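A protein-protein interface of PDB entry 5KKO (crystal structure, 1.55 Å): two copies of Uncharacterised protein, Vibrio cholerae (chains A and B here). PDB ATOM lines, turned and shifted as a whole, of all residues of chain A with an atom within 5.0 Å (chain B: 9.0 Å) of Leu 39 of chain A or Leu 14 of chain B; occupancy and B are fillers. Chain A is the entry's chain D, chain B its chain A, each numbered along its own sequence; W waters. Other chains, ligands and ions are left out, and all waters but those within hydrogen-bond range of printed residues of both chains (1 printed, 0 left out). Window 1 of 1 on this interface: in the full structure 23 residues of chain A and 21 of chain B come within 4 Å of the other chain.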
ATOM      1  N   PHE A   7       8.120  31.775   5.946  1.00  0.00           N
ATOM      2  CA  PHE A   7       8.928  32.130   7.108  1.00  0.00           C
ATOM      3  C   PHE A   7      10.139  31.214   7.164  1.00  0.00           C
ATOM      4  O   PHE A   7      10.076  30.072   6.702  1.00  0.00           O
ATOM      5  CB  PHE A   7       8.119  32.003   8.413  1.00  0.00           C
ATOM      6  CG  PHE A   7       6.932  32.939   8.458  1.00  0.00           C
ATOM      7  CD1 PHE A   7       7.048  34.127   9.140  1.00  0.00           C
ATOM      8  CD2 PHE A   7       5.766  32.677   7.792  1.00  0.00           C
ATOM      9  CE1 PHE A   7       6.010  35.047   9.151  1.00  0.00           C
ATOM     10  CE2 PHE A   7       4.698  33.574   7.801  1.00  0.00           C
ATOM     11  CZ  PHE A   7       4.825  34.764   8.529  1.00  0.00           C
ATOM     12  N   MET A  17      12.239  23.148  19.563  1.00  0.00           N
ATOM     13  CA  MET A  17      10.820  22.755  19.577  1.00  0.00           C
ATOM     14  C   MET A  17      10.702  21.224  19.546  1.00  0.00           C
ATOM     15  O   MET A  17       9.929  20.659  20.303  1.00  0.00           O
ATOM     16  CB  MET A  17      10.039  23.337  18.377  1.00  0.00           C
ATOM     17  CG  MET A  17       9.854  24.855  18.506  1.00  0.00           C
ATOM     18  SD  MET A  17       8.693  25.580  17.135  1.00  0.00           S
ATOM     19  CE  MET A  17       9.870  25.298  15.592  1.00  0.00           C
ATOM     20  N   ILE A  35       6.018  25.565  22.788  1.00  0.00           N
ATOM     21  CA  ILE A  35       6.168  25.508  21.345  1.00  0.00           C
ATOM     22  C   ILE A  35       5.442  26.680  20.710  1.00  0.00           C
ATOM     23  O   ILE A  35       5.943  27.281  19.752  1.00  0.00           O
ATOM     24  CB  ILE A  35       5.682  24.146  20.847  1.00  0.00           C
ATOM     25  CG1 ILE A  35       6.769  23.113  21.223  1.00  0.00           C
ATOM     26  CG2 ILE A  35       5.549  24.163  19.267  1.00  0.00           C
ATOM     27  CD1 ILE A  35       6.371  21.589  21.233  1.00  0.00           C
ATOM     28  N   LYS A  36       4.243  26.993  21.200  1.00  0.00           N
ATOM     29  CA  LYS A  36       3.480  28.129  20.681  1.00  0.00           C
ATOM     30  C   LYS A  36       4.273  29.426  20.772  1.00  0.00           C
ATOM     31  O   LYS A  36       4.288  30.215  19.815  1.00  0.00           O
ATOM     32  CB  LYS A  36       2.133  28.233  21.424  1.00  0.00           C
ATOM     33  CG  LYS A  36       1.303  29.375  20.932  1.00  0.00           C
ATOM     34  CD  LYS A  36      -0.088  29.328  21.524  1.00  0.00           C
ATOM     35  CE  LYS A  36      -0.925  30.417  20.930  1.00  0.00           C
ATOM     36  NZ  LYS A  36      -2.323  30.450  21.520  1.00  0.00           N
ATOM     37  N   ALA A  37       4.944  29.655  21.895  1.00  0.00           N
ATOM     38  CA  ALA A  37       5.780  30.840  22.020  1.00  0.00           C
ATOM     39  C   ALA A  37       6.832  30.906  20.908  1.00  0.00           C
ATOM     40  O   ALA A  37       7.092  31.995  20.352  1.00  0.00           O
ATOM     41  CB  ALA A  37       6.417  30.851  23.404  1.00  0.00           C
ATOM     42  N   HIS A  38       7.517  29.775  20.639  1.00  0.00           N
ATOM     43  CA  HIS A  38       8.529  29.773  19.567  1.00  0.00           C
ATOM     44  C   HIS A  38       7.903  30.042  18.199  1.00  0.00           C
ATOM     45  O   HIS A  38       8.463  30.804  17.398  1.00  0.00           O
ATOM     46  CB  HIS A  38       9.287  28.438  19.542  1.00  0.00           C
ATOM     47  CG  HIS A  38      10.359  28.339  20.587  1.00  0.00           C
ATOM     48  ND1 HIS A  38      10.219  27.615  21.755  1.00  0.00           N
ATOM     49  CD2 HIS A  38      11.577  28.924  20.649  1.00  0.00           C
ATOM     50  CE1 HIS A  38      11.327  27.718  22.467  1.00  0.00           C
ATOM     51  NE2 HIS A  38      12.155  28.525  21.831  1.00  0.00           N
ATOM     52  N   LEU A  39       6.735  29.423  17.928  1.00  0.00           N
ATOM     53  CA  LEU A  39       6.050  29.672  16.666  1.00  0.00           C
ATOM     54  C   LEU A  39       5.601  31.123  16.530  1.00  0.00           C
ATOM     55  O   LEU A  39       5.782  31.736  15.456  1.00  0.00           O
ATOM     56  CB  LEU A  39       4.847  28.746  16.525  1.00  0.00           C
ATOM     57  CG  LEU A  39       5.129  27.254  16.464  1.00  0.00           C
ATOM     58  CD1 LEU A  39       3.791  26.481  16.649  1.00  0.00           C
ATOM     59  CD2 LEU A  39       5.866  26.880  15.188  1.00  0.00           C
ATOM     60  N   LEU A  40       5.102  31.726  17.634  1.00  0.00           N
ATOM     61  CA  LEU A  40       4.733  33.131  17.557  1.00  0.00           C
ATOM     62  C   LEU A  40       5.964  33.997  17.339  1.00  0.00           C
ATOM     63  O   LEU A  40       5.877  35.051  16.691  1.00  0.00           O
ATOM     64  CB  LEU A  40       4.026  33.590  18.844  1.00  0.00           C
ATOM     65  CG  LEU A  40       2.620  33.088  18.982  1.00  0.00           C
ATOM     66  CD1 LEU A  40       2.131  33.218  20.475  1.00  0.00           C
ATOM     67  CD2 LEU A  40       1.734  33.883  18.057  1.00  0.00           C
ATOM     68  N   ASN A  41       7.117  33.596  17.906  1.00  0.00           N
ATOM     69  CA  ASN A  41       8.352  34.358  17.682  1.00  0.00           C
ATOM     70  C   ASN A  41       8.802  34.324  16.223  1.00  0.00           C
ATOM     71  O   ASN A  41       9.294  35.319  15.690  1.00  0.00           O
ATOM     72  CB  ASN A  41       9.413  33.769  18.578  1.00  0.00           C
ATOM     73  CG  ASN A  41      10.478  34.727  18.893  1.00  0.00           C
ATOM     74  OD1 ASN A  41      11.631  34.346  18.994  1.00  0.00           O
ATOM     75  ND2 ASN A  41      10.107  35.987  19.044  1.00  0.00           N
ATOM     76  N   ILE A  42       8.624  33.177  15.574  1.00  0.00           N
ATOM     77  CA  ILE A  42       8.929  33.059  14.149  1.00  0.00           C
ATOM     78  C   ILE A  42       8.014  33.973  13.353  1.00  0.00           C
ATOM     79  O   ILE A  42       8.449  34.715  12.463  1.00  0.00           O
ATOM     80  CB  ILE A  42       8.768  31.577  13.737  1.00  0.00           C
ATOM     81  CG1 ILE A  42       9.895  30.712  14.323  1.00  0.00           C
ATOM     82  CG2 ILE A  42       8.758  31.446  12.215  1.00  0.00           C
ATOM     83  CD1 ILE A  42       9.472  29.192  14.536  1.00  0.00           C
ATOM     84  N   LYS A  43       6.721  33.946  13.696  1.00  0.00           N
ATOM     85  CA  LYS A  43       5.703  34.644  12.912  1.00  0.00           C
ATOM     86  C   LYS A  43       5.785  36.166  13.069  1.00  0.00           C
ATOM     87  O   LYS A  43       5.574  36.900  12.099  1.00  0.00           O
ATOM     88  CB  LYS A  43       4.304  34.154  13.350  1.00  0.00           C
ATOM     89  CG  LYS A  43       3.222  34.841  12.558  1.00  0.00           C
ATOM     90  CD  LYS A  43       1.855  34.633  13.123  1.00  0.00           C
ATOM     91  CE  LYS A  43       0.840  35.205  12.146  1.00  0.00           C
ATOM     92  NZ  LYS A  43      -0.528  34.744  12.481  1.00  0.00           N
ATOM     93  N   PHE B   7      15.050  26.631   7.764  1.00  0.00           N
ATOM     94  CA  PHE B   7      13.999  25.829   7.170  1.00  0.00           C
ATOM     95  C   PHE B   7      12.807  26.723   6.834  1.00  0.00           C
ATOM     96  O   PHE B   7      12.312  27.495   7.673  1.00  0.00           O
ATOM     97  CB  PHE B   7      13.553  24.723   8.169  1.00  0.00           C
ATOM     98  CG  PHE B   7      14.657  23.789   8.582  1.00  0.00           C
ATOM     99  CD1 PHE B   7      15.584  24.140   9.571  1.00  0.00           C
ATOM    100  CD2 PHE B   7      14.768  22.563   8.001  1.00  0.00           C
ATOM    101  CE1 PHE B   7      16.645  23.263   9.923  1.00  0.00           C
ATOM    102  CE2 PHE B   7      15.796  21.667   8.344  1.00  0.00           C
ATOM    103  CZ  PHE B   7      16.737  21.993   9.303  1.00  0.00           C
ATOM    104  N   GLN B   8      12.256  26.528   5.660  1.00  0.00           N
ATOM    105  CA  GLN B   8      11.122  27.319   5.201  1.00  0.00           C
ATOM    106  C   GLN B   8       9.815  26.690   5.644  1.00  0.00           C
ATOM    107  O   GLN B   8       9.654  25.465   5.611  1.00  0.00           O
ATOM    108  CB  GLN B   8      11.100  27.400   3.675  1.00  0.00           C
ATOM    109  CG  GLN B   8      12.338  27.806   2.981  1.00  0.00           C
ATOM    110  CD  GLN B   8      12.051  27.949   1.494  1.00  0.00           C
ATOM    111  OE1 GLN B   8      12.961  28.084   0.680  1.00  0.00           O
ATOM    112  NE2 GLN B   8      10.767  27.917   1.134  1.00  0.00           N
ATOM    113  N   ILE B   9       8.876  27.519   6.067  1.00  0.00           N
ATOM    114  CA  ILE B   9       7.521  27.058   6.364  1.00  0.00           C
ATOM    115  C   ILE B   9       6.559  28.068   5.741  1.00  0.00           C
ATOM    116  O   ILE B   9       6.779  29.286   5.819  1.00  0.00           O
ATOM    117  CB  ILE B   9       7.312  26.923   7.888  1.00  0.00           C
ATOM    118  CG1 ILE B   9       5.970  26.264   8.209  1.00  0.00           C
ATOM    119  CG2 ILE B   9       7.361  28.263   8.549  1.00  0.00           C
ATOM    120  CD1 ILE B   9       5.718  26.074   9.687  1.00  0.00           C
ATOM    121  N   ASP B  10       5.516  27.565   5.077  1.00  0.00           N
ATOM    122  CA  ASP B  10       4.523  28.461   4.528  1.00  0.00           C
ATOM    123  C   ASP B  10       3.660  29.052   5.626  1.00  0.00           C
ATOM    124  O   ASP B  10       3.481  28.465   6.694  1.00  0.00           O
ATOM    125  CB  ASP B  10       3.648  27.708   3.535  1.00  0.00           C
ATOM    126  CG  ASP B  10       3.031  26.476   4.151  1.00  0.00           C
ATOM    127  OD1 ASP B  10       1.819  26.523   4.402  1.00  0.00           O
ATOM    128  OD2 ASP B  10       3.782  25.485   4.377  1.00  0.00           O
ATOM    129  N   GLU B  11       3.088  30.223   5.328  1.00  0.00           N
ATOM    130  CA  GLU B  11       2.297  30.937   6.331  1.00  0.00           C
ATOM    131  C   GLU B  11       1.090  30.136   6.797  1.00  0.00           C
ATOM    132  O   GLU B  11       0.748  30.154   7.984  1.00  0.00           O
ATOM    133  CB  GLU B  11       1.837  32.301   5.790  1.00  0.00           C
ATOM    134  CG  GLU B  11       0.888  33.020   6.745  1.00  0.00           C
ATOM    135  CD  GLU B  11       0.957  34.542   6.707  1.00  0.00           C
ATOM    136  OE1 GLU B  11       0.944  35.156   7.818  1.00  0.00           O
ATOM    137  OE2 GLU B  11       1.019  35.115   5.591  1.00  0.00           O
ATOM    138  N   LEU B  12       0.399  29.448   5.884  1.00  0.00           N
ATOM    139  CA  LEU B  12      -0.789  28.705   6.296  1.00  0.00           C
ATOM    140  C   LEU B  12      -0.437  27.599   7.289  1.00  0.00           C
ATOM    141  O   LEU B  12      -1.115  27.424   8.306  1.00  0.00           O
ATOM    142  CB  LEU B  12      -1.485  28.170   5.036  1.00  0.00           C
ATOM    143  CG  LEU B  12      -2.566  27.127   5.249  1.00  0.00           C
ATOM    144  CD1 LEU B  12      -3.664  27.735   6.118  1.00  0.00           C
ATOM    145  CD2 LEU B  12      -3.143  26.677   3.900  1.00  0.00           C
ATOM    146  N   THR B  13       0.635  26.849   7.026  1.00  0.00           N
ATOM    147  CA  THR B  13       1.011  25.781   7.938  1.00  0.00           C
ATOM    148  C   THR B  13       1.438  26.321   9.303  1.00  0.00           C
ATOM    149  O   THR B  13       1.115  25.734  10.349  1.00  0.00           O
ATOM    150  CB  THR B  13       2.119  24.954   7.316  1.00  0.00           C
ATOM    151  OG1 THR B  13       1.592  24.321   6.143  1.00  0.00           O
ATOM    152  CG2 THR B  13       2.490  23.771   8.254  1.00  0.00           C
ATOM    153  N   LEU B  14       2.155  27.433   9.310  1.00  0.00           N
ATOM    154  CA  LEU B  14       2.562  28.035  10.569  1.00  0.00           C
ATOM    155  C   LEU B  14       1.333  28.472  11.358  1.00  0.00           C
ATOM    156  O   LEU B  14       1.244  28.173  12.566  1.00  0.00           O
ATOM    157  CB  LEU B  14       3.548  29.177  10.309  1.00  0.00           C
ATOM    158  CG  LEU B  14       3.931  30.077  11.481  1.00  0.00           C
ATOM    159  CD1 LEU B  14       4.682  29.165  12.287  1.00  0.00           C
ATOM    160  CD2 LEU B  14       4.859  31.165  10.913  1.00  0.00           C
ATOM    161  N   ASN B  15       0.396  29.188  10.709  1.00  0.00           N
ATOM    162  CA  ASN B  15      -0.855  29.551  11.364  1.00  0.00           C
ATOM    163  C   ASN B  15      -1.615  28.330  11.881  1.00  0.00           C
ATOM    164  O   ASN B  15      -2.212  28.378  12.982  1.00  0.00           O
ATOM    165  CB  ASN B  15      -1.747  30.332  10.391  1.00  0.00           C
ATOM    166  CG  ASN B  15      -1.349  31.736  10.238  1.00  0.00           C
ATOM    167  OD1 ASN B  15      -0.633  32.301  11.080  1.00  0.00           O
ATOM    168  ND2 ASN B  15      -1.831  32.360   9.150  1.00  0.00           N
ATOM    169  N   ALA B  16      -1.685  27.252  11.084  1.00  0.00           N
ATOM    170  CA  ALA B  16      -2.398  26.055  11.541  1.00  0.00           C
ATOM    171  C   ALA B  16      -1.725  25.440  12.758  1.00  0.00           C
ATOM    172  O   ALA B  16      -2.405  25.052  13.720  1.00  0.00           O
ATOM    173  CB  ALA B  16      -2.511  25.003  10.409  1.00  0.00           C
ATOM    174  N   MET B  17      -0.383  25.400  12.776  1.00  0.00           N
ATOM    175  CA  MET B  17       0.308  24.847  13.963  1.00  0.00           C
ATOM    176  C   MET B  17       0.005  25.715  15.180  1.00  0.00           C
ATOM    177  O   MET B  17      -0.271  25.189  16.259  1.00  0.00           O
ATOM    178  CB  MET B  17       1.837  24.826  13.733  1.00  0.00           C
ATOM    179  CG  MET B  17       2.227  23.788  12.747  1.00  0.00           C
ATOM    180  SD  MET B  17       4.121  23.851  12.319  1.00  0.00           S
ATOM    181  CE  MET B  17       4.754  23.127  14.017  1.00  0.00           C
ATOM    182  N   LEU B  18      -0.013  27.036  15.038  1.00  0.00           N
ATOM    183  CA  LEU B  18      -0.397  27.889  16.188  1.00  0.00           C
ATOM    184  C   LEU B  18      -1.771  27.502  16.753  1.00  0.00           C
ATOM    185  O   LEU B  18      -1.964  27.393  17.980  1.00  0.00           O
ATOM    186  CB  LEU B  18      -0.383  29.351  15.759  1.00  0.00           C
ATOM    187  CG  LEU B  18       1.022  29.946  15.645  1.00  0.00           C
ATOM    188  CD1 LEU B  18       0.954  31.298  15.016  1.00  0.00           C
ATOM    189  CD2 LEU B  18       1.635  30.181  17.030  1.00  0.00           C
ATOM    190  N   ARG B  19      -2.754  27.297  15.863  1.00  0.00           N
ATOM    191  CA  ARG B  19      -4.097  26.962  16.316  1.00  0.00           C
ATOM    192  C   ARG B  19      -4.164  25.549  16.849  1.00  0.00           C
ATOM    193  O   ARG B  19      -4.921  25.286  17.809  1.00  0.00           O
ATOM    194  CB  ARG B  19      -5.038  27.090  15.114  1.00  0.00           C
ATOM    195  CG  ARG B  19      -5.250  28.531  14.663  1.00  0.00           C
ATOM    196  CD  ARG B  19      -6.182  29.186  15.665  1.00  0.00           C
ATOM    197  NE  ARG B  19      -6.163  30.638  15.588  1.00  0.00           N
ATOM    198  CZ  ARG B  19      -7.106  31.366  15.014  1.00  0.00           C
ATOM    199  NH1 ARG B  19      -8.150  30.763  14.456  1.00  0.00           N
ATOM    200  NH2 ARG B  19      -7.007  32.696  15.016  1.00  0.00           N
ATOM    201  N   ILE B  20      -3.393  24.626  16.246  1.00  0.00           N
ATOM    202  CA  ILE B  20      -3.417  23.228  16.705  1.00  0.00           C
ATOM    203  C   ILE B  20      -2.990  23.149  18.150  1.00  0.00           C
ATOM    204  O   ILE B  20      -3.444  22.269  18.874  1.00  0.00           O
ATOM    205  CB  ILE B  20      -2.526  22.364  15.791  1.00  0.00           C
ATOM    206  CG1 ILE B  20      -3.268  22.134  14.437  1.00  0.00           C
ATOM    207  CG2 ILE B  20      -2.243  20.988  16.467  1.00  0.00           C
ATOM    208  CD1 ILE B  20      -2.323  21.492  13.363  1.00  0.00           C
ATOM    209  N   THR B  21      -2.107  24.040  18.595  1.00  0.00           N
ATOM    210  CA  THR B  21      -1.624  23.934  19.968  1.00  0.00           C
ATOM    211  C   THR B  21      -2.739  24.067  20.995  1.00  0.00           C
ATOM    212  O   THR B  21      -2.552  23.645  22.154  1.00  0.00           O
ATOM    213  CB  THR B  21      -0.540  24.974  20.346  1.00  0.00           C
ATOM    214  OG1 THR B  21      -1.006  26.339  20.270  1.00  0.00           O
ATOM    215  CG2 THR B  21       0.752  24.803  19.585  1.00  0.00           C
ATOM    216  N   THR B  22      -3.860  24.694  20.645  1.00  0.00           N
ATOM    217  CA  THR B  22      -4.922  24.842  21.616  1.00  0.00           C
ATOM    218  C   THR B  22      -6.282  24.292  21.219  1.00  0.00           C
ATOM    219  O   THR B  22      -7.230  24.511  22.003  1.00  0.00           O
ATOM    220  CB  THR B  22      -5.105  26.322  21.994  1.00  0.00           C
ATOM    221  OG1 THR B  22      -5.508  27.096  20.846  1.00  0.00           O
ATOM    222  CG2 THR B  22      -3.798  26.895  22.632  1.00  0.00           C
ATOM    223  N   ILE B  35       1.519  18.318  16.479  1.00  0.00           N
ATOM    224  CA  ILE B  35       2.627  19.288  16.383  1.00  0.00           C
ATOM    225  C   ILE B  35       3.941  18.570  16.061  1.00  0.00           C
ATOM    226  O   ILE B  35       4.716  19.015  15.203  1.00  0.00           O
ATOM    227  CB  ILE B  35       2.749  20.087  17.694  1.00  0.00           C
ATOM    228  CG1 ILE B  35       1.610  21.092  17.818  1.00  0.00           C
ATOM    229  CG2 ILE B  35       4.111  20.826  17.698  1.00  0.00           C
ATOM    230  CD1 ILE B  35       1.508  22.197  16.679  1.00  0.00           C
ATOM    231  N   HIS B  38       4.173  17.721  12.437  1.00  0.00           N
ATOM    232  CA  HIS B  38       4.535  18.909  11.655  1.00  0.00           C
ATOM    233  C   HIS B  38       6.005  19.274  11.779  1.00  0.00           C
ATOM    234  O   HIS B  38       6.634  19.639  10.770  1.00  0.00           O
ATOM    235  CB  HIS B  38       3.704  20.111  12.046  1.00  0.00           C
ATOM    236  CG  HIS B  38       2.362  20.111  11.444  1.00  0.00           C
ATOM    237  ND1 HIS B  38       1.305  19.404  11.978  1.00  0.00           N
ATOM    238  CD2 HIS B  38       1.890  20.735  10.341  1.00  0.00           C
ATOM    239  CE1 HIS B  38       0.234  19.578  11.202  1.00  0.00           C
ATOM    240  NE2 HIS B  38       0.545  20.432  10.239  1.00  0.00           N
ATOM    241  N   LEU B  39       6.558  19.213  12.995  1.00  0.00           N
ATOM    242  CA  LEU B  39       7.977  19.531  13.211  1.00  0.00           C
ATOM    243  C   LEU B  39       8.830  18.539  12.450  1.00  0.00           C
ATOM    244  O   LEU B  39       9.845  18.924  11.843  1.00  0.00           O
ATOM    245  CB  LEU B  39       8.320  19.489  14.715  1.00  0.00           C
ATOM    246  CG  LEU B  39       7.653  20.609  15.547  1.00  0.00           C
ATOM    247  CD1 LEU B  39       7.887  20.335  17.064  1.00  0.00           C
ATOM    248  CD2 LEU B  39       8.246  22.000  15.165  1.00  0.00           C
ATOM    249  N   ILE B  42       9.036  19.501   8.881  1.00  0.00           N
ATOM    250  CA  ILE B  42       9.950  20.607   8.610  1.00  0.00           C
ATOM    251  C   ILE B  42      11.383  20.107   8.577  1.00  0.00           C
ATOM    252  O   ILE B  42      12.113  20.415   7.651  1.00  0.00           O
ATOM    253  CB  ILE B  42       9.778  21.719   9.660  1.00  0.00           C
ATOM    254  CG1 ILE B  42       8.351  22.241   9.633  1.00  0.00           C
ATOM    255  CG2 ILE B  42      10.881  22.828   9.446  1.00  0.00           C
ATOM    256  CD1 ILE B  42       7.949  23.059  10.914  1.00  0.00           C
HETATM  257  O   HOH W   1      -3.588  28.731  19.612  1.00  0.00           O
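Printed residues of chain B within 4 Å of Leu 39 of chain A: Leu 14, Met 17 and Leu 18. Of the printed residues of chain A, Thr 21 of chain B touches Lys 36 (3.4 Å). Of the printed residues of chain A, Leu 39 of chain B touches Met 17. Leu 12 of chain B touches none of the printed residues of chain A. Thr 22 of chain B touches none of the printed residues of chain A. The nearest printed residue of chain A that does not touch Leu 18 of chain B is Ile 35 of chain A (5.9 Å).
Among the printed residues, pairs that only touch across the chains: Phe 7 of chain A with Phe 7 of chain B, Phe 7 of chain A with Gln 8 of chain B, Phe 7 of chain A with Glu 11 of chain B, Phe 7 of chain A with Leu 14 of chain B, Met 17 of chain A with Leu 39 of chain B, Ile 35 of chain A with Ile 35 of chain B, Lys 36 of chain A with Leu 18 of chain B, Lys 36 of chain A with Thr 21 of chain B, Leu 39 of chain A with Leu 14 of chain B, Leu 39 of chain A with Met 17 of chain B, Leu 39 of chain A with Leu 18 of chain B, Leu 40 of chain A with Leu 18 of chain B, Lys 43 of chain A with Leu 14 of chain B and Lys 43 of chain A with Leu 18 of chain B.
N of Phe 7 of chain A lies within hydrogen-bond range of O of Ile 9 of chain B (2.8 Å). The side-chain amide oxygen (OD1) of Asn 15 of chain B lies within hydrogen-bond range of the side-chain amino group (NZ) of Lys 43 of chain A (2.8 Å).
Water W1 lies within hydrogen-bond range of O of Leu 18 of chain B, OG1 of Thr 22 of chain B and NZ of Lys 36 of chain A.
The backbone carbonyl oxygen (O) of Leu 18 of chain B lies within hydrogen-bond range of the side-chain hydroxyl (OG1) of Thr 21 of chain B, at 2.7 Å.
Of the 11 printed residues of chain A, 7 touch a printed residue of chain B. Hydrophobic or aromatic side chains of chain B within 4 Å of the printed part of chain A: Ile 9, Leu 14, Met 17, Leu 18, Ile 35 and Leu 39. Among the printed residues, 16 pairs touch across the chains. Among the printed residues, no Asp or Glu carboxylate lies within 4 Å of a Lys or Arg side-chain nitrogen of the other chain.
Phe 7 of chain A touches its own counterpart, Phe 7 of chain B. Met 17 of chain A touches Leu 39 of chain B, and with the chains exchanged Leu 39 of chain A touches Met 17 of chain B. Ile 35 of chain A touches its own counterpart, Ile 35 of chain B. Positions printed for both chains: 7, 17, 35, 38, 39 and 42. Of the 16 pairs that touch across the chains among the printed residues, 4 have their exchanged pair printed and touching as well.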
